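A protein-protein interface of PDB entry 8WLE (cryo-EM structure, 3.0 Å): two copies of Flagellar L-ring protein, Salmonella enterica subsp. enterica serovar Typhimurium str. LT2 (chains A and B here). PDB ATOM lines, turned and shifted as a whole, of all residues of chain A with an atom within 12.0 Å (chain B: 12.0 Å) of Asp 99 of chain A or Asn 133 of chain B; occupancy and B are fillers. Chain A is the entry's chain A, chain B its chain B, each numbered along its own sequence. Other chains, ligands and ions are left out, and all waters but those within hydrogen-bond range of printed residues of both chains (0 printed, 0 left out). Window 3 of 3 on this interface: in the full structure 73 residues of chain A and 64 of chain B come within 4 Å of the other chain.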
ATOM      1  N   ASN A  95     -15.553  41.110 -38.235  1.00  0.00           N
ATOM      2  CA  ASN A  95     -16.056  39.746 -38.184  1.00  0.00           C
ATOM      3  C   ASN A  95     -16.562  39.440 -36.786  1.00  0.00           C
ATOM      4  O   ASN A  95     -16.217  40.113 -35.813  1.00  0.00           O
ATOM      5  CB  ASN A  95     -14.988  38.729 -38.602  1.00  0.00           C
ATOM      6  CG  ASN A  95     -13.734  38.822 -37.770  1.00  0.00           C
ATOM      7  OD1 ASN A  95     -12.800  39.542 -38.117  1.00  0.00           O
ATOM      8  ND2 ASN A  95     -13.700  38.087 -36.666  1.00  0.00           N
ATOM      9  N   ALA A  96     -17.403  38.414 -36.709  1.00  0.00           N
ATOM     10  CA  ALA A  96     -17.904  37.917 -35.439  1.00  0.00           C
ATOM     11  C   ALA A  96     -18.267  36.454 -35.608  1.00  0.00           C
ATOM     12  O   ALA A  96     -18.648  36.018 -36.696  1.00  0.00           O
ATOM     13  CB  ALA A  96     -19.115  38.716 -34.953  1.00  0.00           C
ATOM     14  N   SER A  97     -18.134  35.694 -34.526  1.00  0.00           N
ATOM     15  CA  SER A  97     -18.484  34.283 -34.546  1.00  0.00           C
ATOM     16  C   SER A  97     -18.946  33.880 -33.155  1.00  0.00           C
ATOM     17  O   SER A  97     -18.608  34.519 -32.159  1.00  0.00           O
ATOM     18  CB  SER A  97     -17.301  33.423 -35.004  1.00  0.00           C
ATOM     19  OG  SER A  97     -17.699  32.091 -35.262  1.00  0.00           O
ATOM     20  N   ARG A  98     -19.736  32.811 -33.101  1.00  0.00           N
ATOM     21  CA  ARG A  98     -20.232  32.295 -31.829  1.00  0.00           C
ATOM     22  C   ARG A  98     -20.681  30.859 -32.043  1.00  0.00           C
ATOM     23  O   ARG A  98     -21.546  30.605 -32.884  1.00  0.00           O
ATOM     24  CB  ARG A  98     -21.382  33.153 -31.306  1.00  0.00           C
ATOM     25  CG  ARG A  98     -21.629  33.006 -29.820  1.00  0.00           C
ATOM     26  CD  ARG A  98     -22.698  33.964 -29.333  1.00  0.00           C
ATOM     27  NE  ARG A  98     -24.035  33.553 -29.738  1.00  0.00           N
ATOM     28  CZ  ARG A  98     -25.148  34.168 -29.365  1.00  0.00           C
ATOM     29  NH1 ARG A  98     -25.119  35.227 -28.575  1.00  0.00           N
ATOM     30  NH2 ARG A  98     -26.319  33.709 -29.795  1.00  0.00           N
ATOM     31  N   ASP A  99     -20.097  29.925 -31.296  1.00  0.00           N
ATOM     32  CA  ASP A  99     -20.427  28.510 -31.402  1.00  0.00           C
ATOM     33  C   ASP A  99     -20.763  27.967 -30.025  1.00  0.00           C
ATOM     34  O   ASP A  99     -20.100  28.311 -29.043  1.00  0.00           O
ATOM     35  CB  ASP A  99     -19.275  27.706 -32.005  1.00  0.00           C
ATOM     36  CG  ASP A  99     -19.243  27.776 -33.515  1.00  0.00           C
ATOM     37  OD1 ASP A  99     -19.859  28.699 -34.085  1.00  0.00           O
ATOM     38  OD2 ASP A  99     -18.606  26.897 -34.134  1.00  0.00           O
ATOM     39  N   GLY A 100     -21.788  27.122 -29.955  1.00  0.00           N
ATOM     40  CA  GLY A 100     -22.169  26.518 -28.696  1.00  0.00           C
ATOM     41  C   GLY A 100     -22.713  25.115 -28.844  1.00  0.00           C
ATOM     42  O   GLY A 100     -23.478  24.836 -29.770  1.00  0.00           O
ATOM     43  N   LYS A 101     -22.314  24.220 -27.947  1.00  0.00           N
ATOM     44  CA  LYS A 101     -22.865  22.877 -27.867  1.00  0.00           C
ATOM     45  C   LYS A 101     -23.204  22.573 -26.419  1.00  0.00           C
ATOM     46  O   LYS A 101     -22.499  23.009 -25.506  1.00  0.00           O
ATOM     47  CB  LYS A 101     -21.890  21.831 -28.402  1.00  0.00           C
ATOM     48  CG  LYS A 101     -21.582  21.966 -29.876  1.00  0.00           C
ATOM     49  CD  LYS A 101     -20.597  20.900 -30.331  1.00  0.00           C
ATOM     50  CE  LYS A 101     -20.261  21.056 -31.805  1.00  0.00           C
ATOM     51  NZ  LYS A 101     -19.329  19.996 -32.280  1.00  0.00           N
ATOM     52  N   THR A 102     -24.287  21.834 -26.214  1.00  0.00           N
ATOM     53  CA  THR A 102     -24.701  21.404 -24.889  1.00  0.00           C
ATOM     54  C   THR A 102     -25.217  19.979 -24.995  1.00  0.00           C
ATOM     55  O   THR A 102     -25.857  19.616 -25.982  1.00  0.00           O
ATOM     56  CB  THR A 102     -25.789  22.320 -24.309  1.00  0.00           C
ATOM     57  OG1 THR A 102     -25.394  23.689 -24.460  1.00  0.00           O
ATOM     58  CG2 THR A 102     -26.007  22.030 -22.836  1.00  0.00           C
ATOM     59  N   SER A 103     -24.931  19.172 -23.977  1.00  0.00           N
ATOM     60  CA  SER A 103     -25.378  17.789 -23.980  1.00  0.00           C
ATOM     61  C   SER A 103     -25.463  17.275 -22.553  1.00  0.00           C
ATOM     62  O   SER A 103     -24.699  17.691 -21.679  1.00  0.00           O
ATOM     63  CB  SER A 103     -24.442  16.897 -24.801  1.00  0.00           C
ATOM     64  OG  SER A 103     -24.425  17.297 -26.158  1.00  0.00           O
ATOM     65  N   ALA A 126     -28.107  20.002 -27.763  1.00  0.00           N
ATOM     66  CA  ALA A 126     -28.428  21.200 -28.522  1.00  0.00           C
ATOM     67  C   ALA A 126     -27.155  21.823 -29.071  1.00  0.00           C
ATOM     68  O   ALA A 126     -26.077  21.685 -28.493  1.00  0.00           O
ATOM     69  CB  ALA A 126     -29.177  22.224 -27.667  1.00  0.00           C
ATOM     70  N   SER A 127     -27.288  22.510 -30.201  1.00  0.00           N
ATOM     71  CA  SER A 127     -26.158  23.168 -30.840  1.00  0.00           C
ATOM     72  C   SER A 127     -26.614  24.483 -31.450  1.00  0.00           C
ATOM     73  O   SER A 127     -27.781  24.649 -31.807  1.00  0.00           O
ATOM     74  CB  SER A 127     -25.528  22.287 -31.921  1.00  0.00           C
ATOM     75  OG  SER A 127     -24.391  22.911 -32.484  1.00  0.00           O
ATOM     76  N   GLY A 128     -25.679  25.419 -31.562  1.00  0.00           N
ATOM     77  CA  GLY A 128     -25.974  26.703 -32.166  1.00  0.00           C
ATOM     78  C   GLY A 128     -24.716  27.338 -32.713  1.00  0.00           C
ATOM     79  O   GLY A 128     -23.609  27.104 -32.219  1.00  0.00           O
ATOM     80  N   GLY A 129     -24.900  28.159 -33.738  1.00  0.00           N
ATOM     81  CA  GLY A 129     -23.779  28.831 -34.366  1.00  0.00           C
ATOM     82  C   GLY A 129     -24.224  30.064 -35.101  1.00  0.00           C
ATOM     83  O   GLY A 129     -25.302  30.102 -35.704  1.00  0.00           O
ATOM     84  N   ASN A 130     -23.381  31.091 -35.063  1.00  0.00           N
ATOM     85  CA  ASN A 130     -23.646  32.347 -35.744  1.00  0.00           C
ATOM     86  C   ASN A 130     -22.319  32.906 -36.222  1.00  0.00           C
ATOM     87  O   ASN A 130     -21.332  32.864 -35.486  1.00  0.00           O
ATOM     88  CB  ASN A 130     -24.344  33.345 -34.820  1.00  0.00           C
ATOM     89  CG  ASN A 130     -25.097  34.412 -35.580  1.00  0.00           C
ATOM     90  OD1 ASN A 130     -24.497  35.286 -36.202  1.00  0.00           O
ATOM     91  ND2 ASN A 130     -26.421  34.352 -35.526  1.00  0.00           N
ATOM     92  N   SER A 131     -22.284  33.403 -37.454  1.00  0.00           N
ATOM     93  CA  SER A 131     -21.048  33.895 -38.042  1.00  0.00           C
ATOM     94  C   SER A 131     -21.342  35.095 -38.925  1.00  0.00           C
ATOM     95  O   SER A 131     -22.429  35.213 -39.495  1.00  0.00           O
ATOM     96  CB  SER A 131     -20.343  32.809 -38.857  1.00  0.00           C
ATOM     97  OG  SER A 131     -19.278  33.358 -39.609  1.00  0.00           O
ATOM     98  N   PHE A 132     -20.357  35.981 -39.034  1.00  0.00           N
ATOM     99  CA  PHE A 132     -20.474  37.156 -39.883  1.00  0.00           C
ATOM    100  C   PHE A 132     -19.079  37.631 -40.247  1.00  0.00           C
ATOM    101  O   PHE A 132     -18.180  37.617 -39.406  1.00  0.00           O
ATOM    102  CB  PHE A 132     -21.246  38.281 -39.192  1.00  0.00           C
ATOM    103  CG  PHE A 132     -21.130  39.598 -39.889  1.00  0.00           C
ATOM    104  CD1 PHE A 132     -21.847  39.844 -41.045  1.00  0.00           C
ATOM    105  CD2 PHE A 132     -20.296  40.584 -39.403  1.00  0.00           C
ATOM    106  CE1 PHE A 132     -21.739  41.047 -41.697  1.00  0.00           C
ATOM    107  CE2 PHE A 132     -20.185  41.792 -40.052  1.00  0.00           C
ATOM    108  CZ  PHE A 132     -20.909  42.023 -41.201  1.00  0.00           C
ATOM    109  N   ASN A 133     -18.918  38.075 -41.492  1.00  0.00           N
ATOM    110  CA  ASN A 133     -17.611  38.465 -42.009  1.00  0.00           C
ATOM    111  C   ASN A 133     -17.835  39.505 -43.097  1.00  0.00           C
ATOM    112  O   ASN A 133     -18.188  39.152 -44.224  1.00  0.00           O
ATOM    113  CB  ASN A 133     -16.867  37.249 -42.555  1.00  0.00           C
ATOM    114  CG  ASN A 133     -15.579  36.976 -41.825  1.00  0.00           C
ATOM    115  OD1 ASN A 133     -14.720  37.849 -41.707  1.00  0.00           O
ATOM    116  ND2 ASN A 133     -15.437  35.758 -41.318  1.00  0.00           N
ATOM    117  N   SER B  92     -10.980  40.359 -30.164  1.00  0.00           N
ATOM    118  CA  SER B  92     -11.307  39.817 -28.856  1.00  0.00           C
ATOM    119  C   SER B  92     -11.897  38.430 -29.038  1.00  0.00           C
ATOM    120  O   SER B  92     -12.373  38.074 -30.119  1.00  0.00           O
ATOM    121  CB  SER B  92     -12.282  40.720 -28.099  1.00  0.00           C
ATOM    122  OG  SER B  92     -13.538  40.757 -28.744  1.00  0.00           O
ATOM    123  N   SER B  93     -11.869  37.659 -27.956  1.00  0.00           N
ATOM    124  CA  SER B  93     -12.443  36.324 -27.964  1.00  0.00           C
ATOM    125  C   SER B  93     -12.774  35.926 -26.536  1.00  0.00           C
ATOM    126  O   SER B  93     -12.301  36.534 -25.576  1.00  0.00           O
ATOM    127  CB  SER B  93     -11.497  35.304 -28.602  1.00  0.00           C
ATOM    128  OG  SER B  93     -10.309  35.171 -27.849  1.00  0.00           O
ATOM    129  N   ALA B  94     -13.607  34.897 -26.419  1.00  0.00           N
ATOM    130  CA  ALA B  94     -13.981  34.321 -25.140  1.00  0.00           C
ATOM    131  C   ALA B  94     -14.391  32.878 -25.380  1.00  0.00           C
ATOM    132  O   ALA B  94     -14.897  32.545 -26.453  1.00  0.00           O
ATOM    133  CB  ALA B  94     -15.123  35.100 -24.482  1.00  0.00           C
ATOM    134  N   ASN B  95     -14.142  32.018 -24.398  1.00  0.00           N
ATOM    135  CA  ASN B  95     -14.544  30.626 -24.528  1.00  0.00           C
ATOM    136  C   ASN B  95     -14.816  30.041 -23.154  1.00  0.00           C
ATOM    137  O   ASN B  95     -14.373  30.565 -22.131  1.00  0.00           O
ATOM    138  CB  ASN B  95     -13.489  29.794 -25.266  1.00  0.00           C
ATOM    139  CG  ASN B  95     -12.134  29.854 -24.608  1.00  0.00           C
ATOM    140  OD1 ASN B  95     -11.309  30.702 -24.943  1.00  0.00           O
ATOM    141  ND2 ASN B  95     -11.889  28.947 -23.673  1.00  0.00           N
ATOM    142  N   ALA B  96     -15.570  28.947 -23.152  1.00  0.00           N
ATOM    143  CA  ALA B  96     -15.843  28.198 -21.939  1.00  0.00           C
ATOM    144  C   ALA B  96     -16.134  26.759 -22.321  1.00  0.00           C
ATOM    145  O   ALA B  96     -16.646  26.484 -23.407  1.00  0.00           O
ATOM    146  CB  ALA B  96     -17.016  28.792 -21.155  1.00  0.00           C
ATOM    147  N   SER B  97     -15.795  25.840 -21.423  1.00  0.00           N
ATOM    148  CA  SER B  97     -16.054  24.428 -21.652  1.00  0.00           C
ATOM    149  C   SER B  97     -16.277  23.753 -20.308  1.00  0.00           C
ATOM    150  O   SER B  97     -15.835  24.240 -19.268  1.00  0.00           O
ATOM    151  CB  SER B  97     -14.901  23.766 -22.416  1.00  0.00           C
ATOM    152  OG  SER B  97     -15.249  22.468 -22.855  1.00  0.00           O
ATOM    153  N   ARG B  98     -16.981  22.625 -20.343  1.00  0.00           N
ATOM    154  CA  ARG B  98     -17.248  21.857 -19.130  1.00  0.00           C
ATOM    155  C   ARG B  98     -17.633  20.445 -19.540  1.00  0.00           C
ATOM    156  O   ARG B  98     -18.596  20.263 -20.287  1.00  0.00           O
ATOM    157  CB  ARG B  98     -18.359  22.508 -18.309  1.00  0.00           C
ATOM    158  CG  ARG B  98     -18.371  22.087 -16.855  1.00  0.00           C
ATOM    159  CD  ARG B  98     -19.414  22.849 -16.061  1.00  0.00           C
ATOM    160  NE  ARG B  98     -20.769  22.397 -16.349  1.00  0.00           N
ATOM    161  CZ  ARG B  98     -21.849  22.838 -15.722  1.00  0.00           C
ATOM    162  NH1 ARG B  98     -21.770  23.745 -14.764  1.00  0.00           N
ATOM    163  NH2 ARG B  98     -23.040  22.357 -16.066  1.00  0.00           N
ATOM    164  N   ASP B  99     -16.886  19.452 -19.062  1.00  0.00           N
ATOM    165  CA  ASP B  99     -17.140  18.053 -19.378  1.00  0.00           C
ATOM    166  C   ASP B  99     -17.231  17.254 -18.091  1.00  0.00           C
ATOM    167  O   ASP B  99     -16.452  17.481 -17.161  1.00  0.00           O
ATOM    168  CB  ASP B  99     -16.043  17.469 -20.268  1.00  0.00           C
ATOM    169  CG  ASP B  99     -16.240  17.799 -21.729  1.00  0.00           C
ATOM    170  OD1 ASP B  99     -16.991  18.747 -22.034  1.00  0.00           O
ATOM    171  OD2 ASP B  99     -15.649  17.099 -22.580  1.00  0.00           O
ATOM    172  N   GLY B 129     -21.880  17.713 -21.109  1.00  0.00           N
ATOM    173  CA  GLY B 129     -20.910  18.579 -21.751  1.00  0.00           C
ATOM    174  C   GLY B 129     -21.536  19.875 -22.181  1.00  0.00           C
ATOM    175  O   GLY B 129     -22.692  19.921 -22.616  1.00  0.00           O
ATOM    176  N   ASN B 130     -20.764  20.952 -22.073  1.00  0.00           N
ATOM    177  CA  ASN B 130     -21.205  22.278 -22.471  1.00  0.00           C
ATOM    178  C   ASN B 130     -20.002  23.024 -23.016  1.00  0.00           C
ATOM    179  O   ASN B 130     -18.916  22.945 -22.439  1.00  0.00           O
ATOM    180  CB  ASN B 130     -21.819  23.036 -21.294  1.00  0.00           C
ATOM    181  CG  ASN B 130     -22.742  24.146 -21.737  1.00  0.00           C
ATOM    182  OD1 ASN B 130     -22.298  25.164 -22.265  1.00  0.00           O
ATOM    183  ND2 ASN B 130     -24.037  23.961 -21.515  1.00  0.00           N
ATOM    184  N   SER B 131     -20.182  23.726 -24.129  1.00  0.00           N
ATOM    185  CA  SER B 131     -19.082  24.419 -24.779  1.00  0.00           C
ATOM    186  C   SER B 131     -19.579  25.721 -25.381  1.00  0.00           C
ATOM    187  O   SER B 131     -20.744  25.839 -25.766  1.00  0.00           O
ATOM    188  CB  SER B 131     -18.440  23.555 -25.866  1.00  0.00           C
ATOM    189  OG  SER B 131     -17.536  24.317 -26.643  1.00  0.00           O
ATOM    190  N   PHE B 132     -18.679  26.697 -25.460  1.00  0.00           N
ATOM    191  CA  PHE B 132     -18.995  27.985 -26.056  1.00  0.00           C
ATOM    192  C   PHE B 132     -17.703  28.637 -26.513  1.00  0.00           C
ATOM    193  O   PHE B 132     -16.689  28.558 -25.818  1.00  0.00           O
ATOM    194  CB  PHE B 132     -19.724  28.901 -25.072  1.00  0.00           C
ATOM    195  CG  PHE B 132     -19.796  30.323 -25.527  1.00  0.00           C
ATOM    196  CD1 PHE B 132     -20.692  30.700 -26.510  1.00  0.00           C
ATOM    197  CD2 PHE B 132     -18.963  31.282 -24.988  1.00  0.00           C
ATOM    198  CE1 PHE B 132     -20.759  32.002 -26.941  1.00  0.00           C
ATOM    199  CE2 PHE B 132     -19.027  32.589 -25.415  1.00  0.00           C
ATOM    200  CZ  PHE B 132     -19.927  32.947 -26.392  1.00  0.00           C
ATOM    201  N   ASN B 133     -17.758  29.300 -27.666  1.00  0.00           N
ATOM    202  CA  ASN B 133     -16.570  29.886 -28.276  1.00  0.00           C
ATOM    203  C   ASN B 133     -17.019  31.073 -29.116  1.00  0.00           C
ATOM    204  O   ASN B 133     -17.514  30.889 -30.230  1.00  0.00           O
ATOM    205  CB  ASN B 133     -15.841  28.853 -29.131  1.00  0.00           C
ATOM    206  CG  ASN B 133     -14.443  28.574 -28.643  1.00  0.00           C
ATOM    207  OD1 ASN B 133     -13.634  29.486 -28.487  1.00  0.00           O
ATOM    208  ND2 ASN B 133     -14.151  27.303 -28.391  1.00  0.00           N
ATOM    209  N   GLY B 134     -16.839  32.279 -28.591  1.00  0.00           N
ATOM    210  CA  GLY B 134     -17.172  33.488 -29.314  1.00  0.00           C
ATOM    211  C   GLY B 134     -15.911  34.271 -29.620  1.00  0.00           C
ATOM    212  O   GLY B 134     -14.929  34.205 -28.883  1.00  0.00           O
ATOM    213  N   LYS B 135     -15.943  35.004 -30.725  1.00  0.00           N
ATOM    214  CA  LYS B 135     -14.805  35.819 -31.118  1.00  0.00           C
ATOM    215  C   LYS B 135     -15.302  36.943 -32.008  1.00  0.00           C
ATOM    216  O   LYS B 135     -16.402  36.885 -32.557  1.00  0.00           O
ATOM    217  CB  LYS B 135     -13.736  34.990 -31.833  1.00  0.00           C
ATOM    218  CG  LYS B 135     -14.261  34.196 -33.009  1.00  0.00           C
ATOM    219  CD  LYS B 135     -13.221  33.217 -33.518  1.00  0.00           C
ATOM    220  CE  LYS B 135     -12.098  33.929 -34.240  1.00  0.00           C
ATOM    221  NZ  LYS B 135     -12.583  34.573 -35.490  1.00  0.00           N
ATOM    222  N   GLY B 136     -14.474  37.969 -32.135  1.00  0.00           N
ATOM    223  CA  GLY B 136     -14.841  39.112 -32.947  1.00  0.00           C
ATOM    224  C   GLY B 136     -13.641  40.002 -33.150  1.00  0.00           C
ATOM    225  O   GLY B 136     -12.588  39.816 -32.535  1.00  0.00           O
ATOM    226  N   GLY B 137     -13.821  40.986 -34.021  1.00  0.00           N
ATOM    227  CA  GLY B 137     -12.749  41.906 -34.318  1.00  0.00           C
ATOM    228  C   GLY B 137     -13.080  42.872 -35.432  1.00  0.00           C
ATOM    229  O   GLY B 137     -14.085  42.717 -36.129  1.00  0.00           O
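The backbone carbonyl oxygen (O) of Gly 100 of chain A sits close to the side-chain hydroxyl (OG) of Ser 127 of chain A (3.5 Å).
N of Arg 98 of chain A sits at hydrogen-bond distance from O of Asn 130 of chain A (2.9 Å).
The backbone NH of Arg 98 of chain B is in hydrogen-bond range of the backbone carbonyl oxygen of Asn 130 of chain B, 2.9 Å away.
The backbone carbonyl oxygen of Ser 92 of chain B lies within hydrogen-bond range of the backbone NH of Gly 136 of chain B, 2.9 Å away.
The backbone NH (N) of Phe 132 of chain A is in hydrogen-bond range of the backbone carbonyl oxygen (O) of Ala 96 of chain A (2.9 Å).
O of Gly 100 of chain A sits at hydrogen-bond distance from N of Gly 128 of chain A.
The backbone carbonyl oxygen (O) of Asp 99 of chain A sits at hydrogen-bond distance from the backbone NH (N) of Asn 133 of chain B (2.9 Å).
The backbone carbonyl oxygen (O) of Lys 101 of chain A lies within hydrogen-bond range of the backbone NH (N) of Ser 131 of chain B, at 2.8 Å.
The backbone NH of Ser 97 of chain A is in hydrogen-bond range of the backbone carbonyl oxygen of Lys 135 of chain B (2.9 Å).
The side-chain hydroxyl of Thr 102 of chain A sits close to the side-chain amide nitrogen of Asn 130 of chain B, 3.3 Å away.
The backbone NH (N) of Ser 103 of chain A lies within hydrogen-bond range of the backbone carbonyl oxygen (O) of Gly 129 of chain B, 2.7 Å away.
O of Gly 137 of chain B lies within hydrogen-bond range of N of Asn 95 of chain A.
Of chain B, only Gly 134 and Lys 135 come within 4 Å of Ser 97 of chain A.
Of chain B, only Phe 132 (3.2 Å) and Asn 133 (3.5 Å) come within 4 Å of Arg 98 of chain A.
Of the printed residues of chain B, Asp 99 of chain A touches Phe 132 (3.2 Å) and Asn 133 (2.9 Å).
Gly 100 of chain A touches just one residue of chain B: Ser 131.
Ala 126 of chain A touches none of the printed residues of chain B.
No residue of chain B comes within 4 Å of Gly 128 of chain A.
No residue of chain B comes within 4 Å of Gly 129 of chain A.
No residue of chain A comes within 4 Å of Ala 94 of chain B.
No residue of chain A comes within 4 Å of Asn 95 of chain B.
No residue of chain A comes within 4 Å of Ala 96 of chain B.
Ser 131 of chain B touches two residues of chain A.
Of the printed residues of chain A, Phe 132 of chain B touches Arg 98 and Asp 99.
Of the printed residues of chain A, Asn 133 of chain B touches Arg 98 (3.5 Å) and Asp 99 (2.9 Å).
Printed residues of chain A within 4 Å of Gly 134 of chain B: Ser 97 (3.3 Å).
Printed residues of chain A within 4 Å of Lys 135 of chain B: Asn 95 (3.9 Å), Ala 96 (3.4 Å) and Ser 97 (2.9 Å).
Of the printed residues of chain A, Gly 137 of chain B touches Asn 95 (3.0 Å).
The nearest printed residue of chain B that does not touch Ser 103 of chain A is Asn 130 of chain B (4.9 Å).
Hydrophobic or aromatic side chains of chain B within 4 Å of the printed part of chain A: Phe 132.
Along chain A the printed residues that touch a printed residue of chain B span positions 95 to 103.
Among the printed residues, 16 pairs touch across the chains.
Among the printed residues, no Asp or Glu carboxylate lies within 4 Å of a Lys or Arg side-chain nitrogen of the other chain.
Among the printed residues, pairs that only touch across the chains: Asn 95 of chain A with Lys 135 of chain B, Asn 95 of chain A with Gly 136 of chain B, Ala 96 of chain A with Lys 135 of chain B, Ser 97 of chain A with Gly 134 of chain B, Arg 98 of chain A with Phe 132 of chain B, Arg 98 of chain A with Asn 133 of chain B, Asp 99 of chain A with Phe 132 of chain B, Gly 100 of chain A with Ser 131 of chain B, Lys 101 of chain A with Asn 130 of chain B and Thr 102 of chain A with Gly 129 of chain B.
Arg 98 of chain A touches Phe 132 of chain B, but with the chains exchanged Phe 132 of chain A does not touch Arg 98 of chain B (23.2 Å).
Arg 98 of chain A touches Asn 133 of chain B, but with the chains exchanged Asn 133 of chain A does not touch Arg 98 of chain B (24.8 Å).
Asp 99 of chain A touches Phe 132 of chain B, but with the chains exchanged Phe 132 of chain A does not touch Asp 99 of chain B (24.4 Å).
Asp 99 of chain A touches Asn 133 of chain B, but with the chains exchanged Asn 133 of chain A does not touch Asp 99 of chain B (25.8 Å).
Of the 16 pairs that touch across the chains among the printed residues, none has its exchanged pair printed and touching as well.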
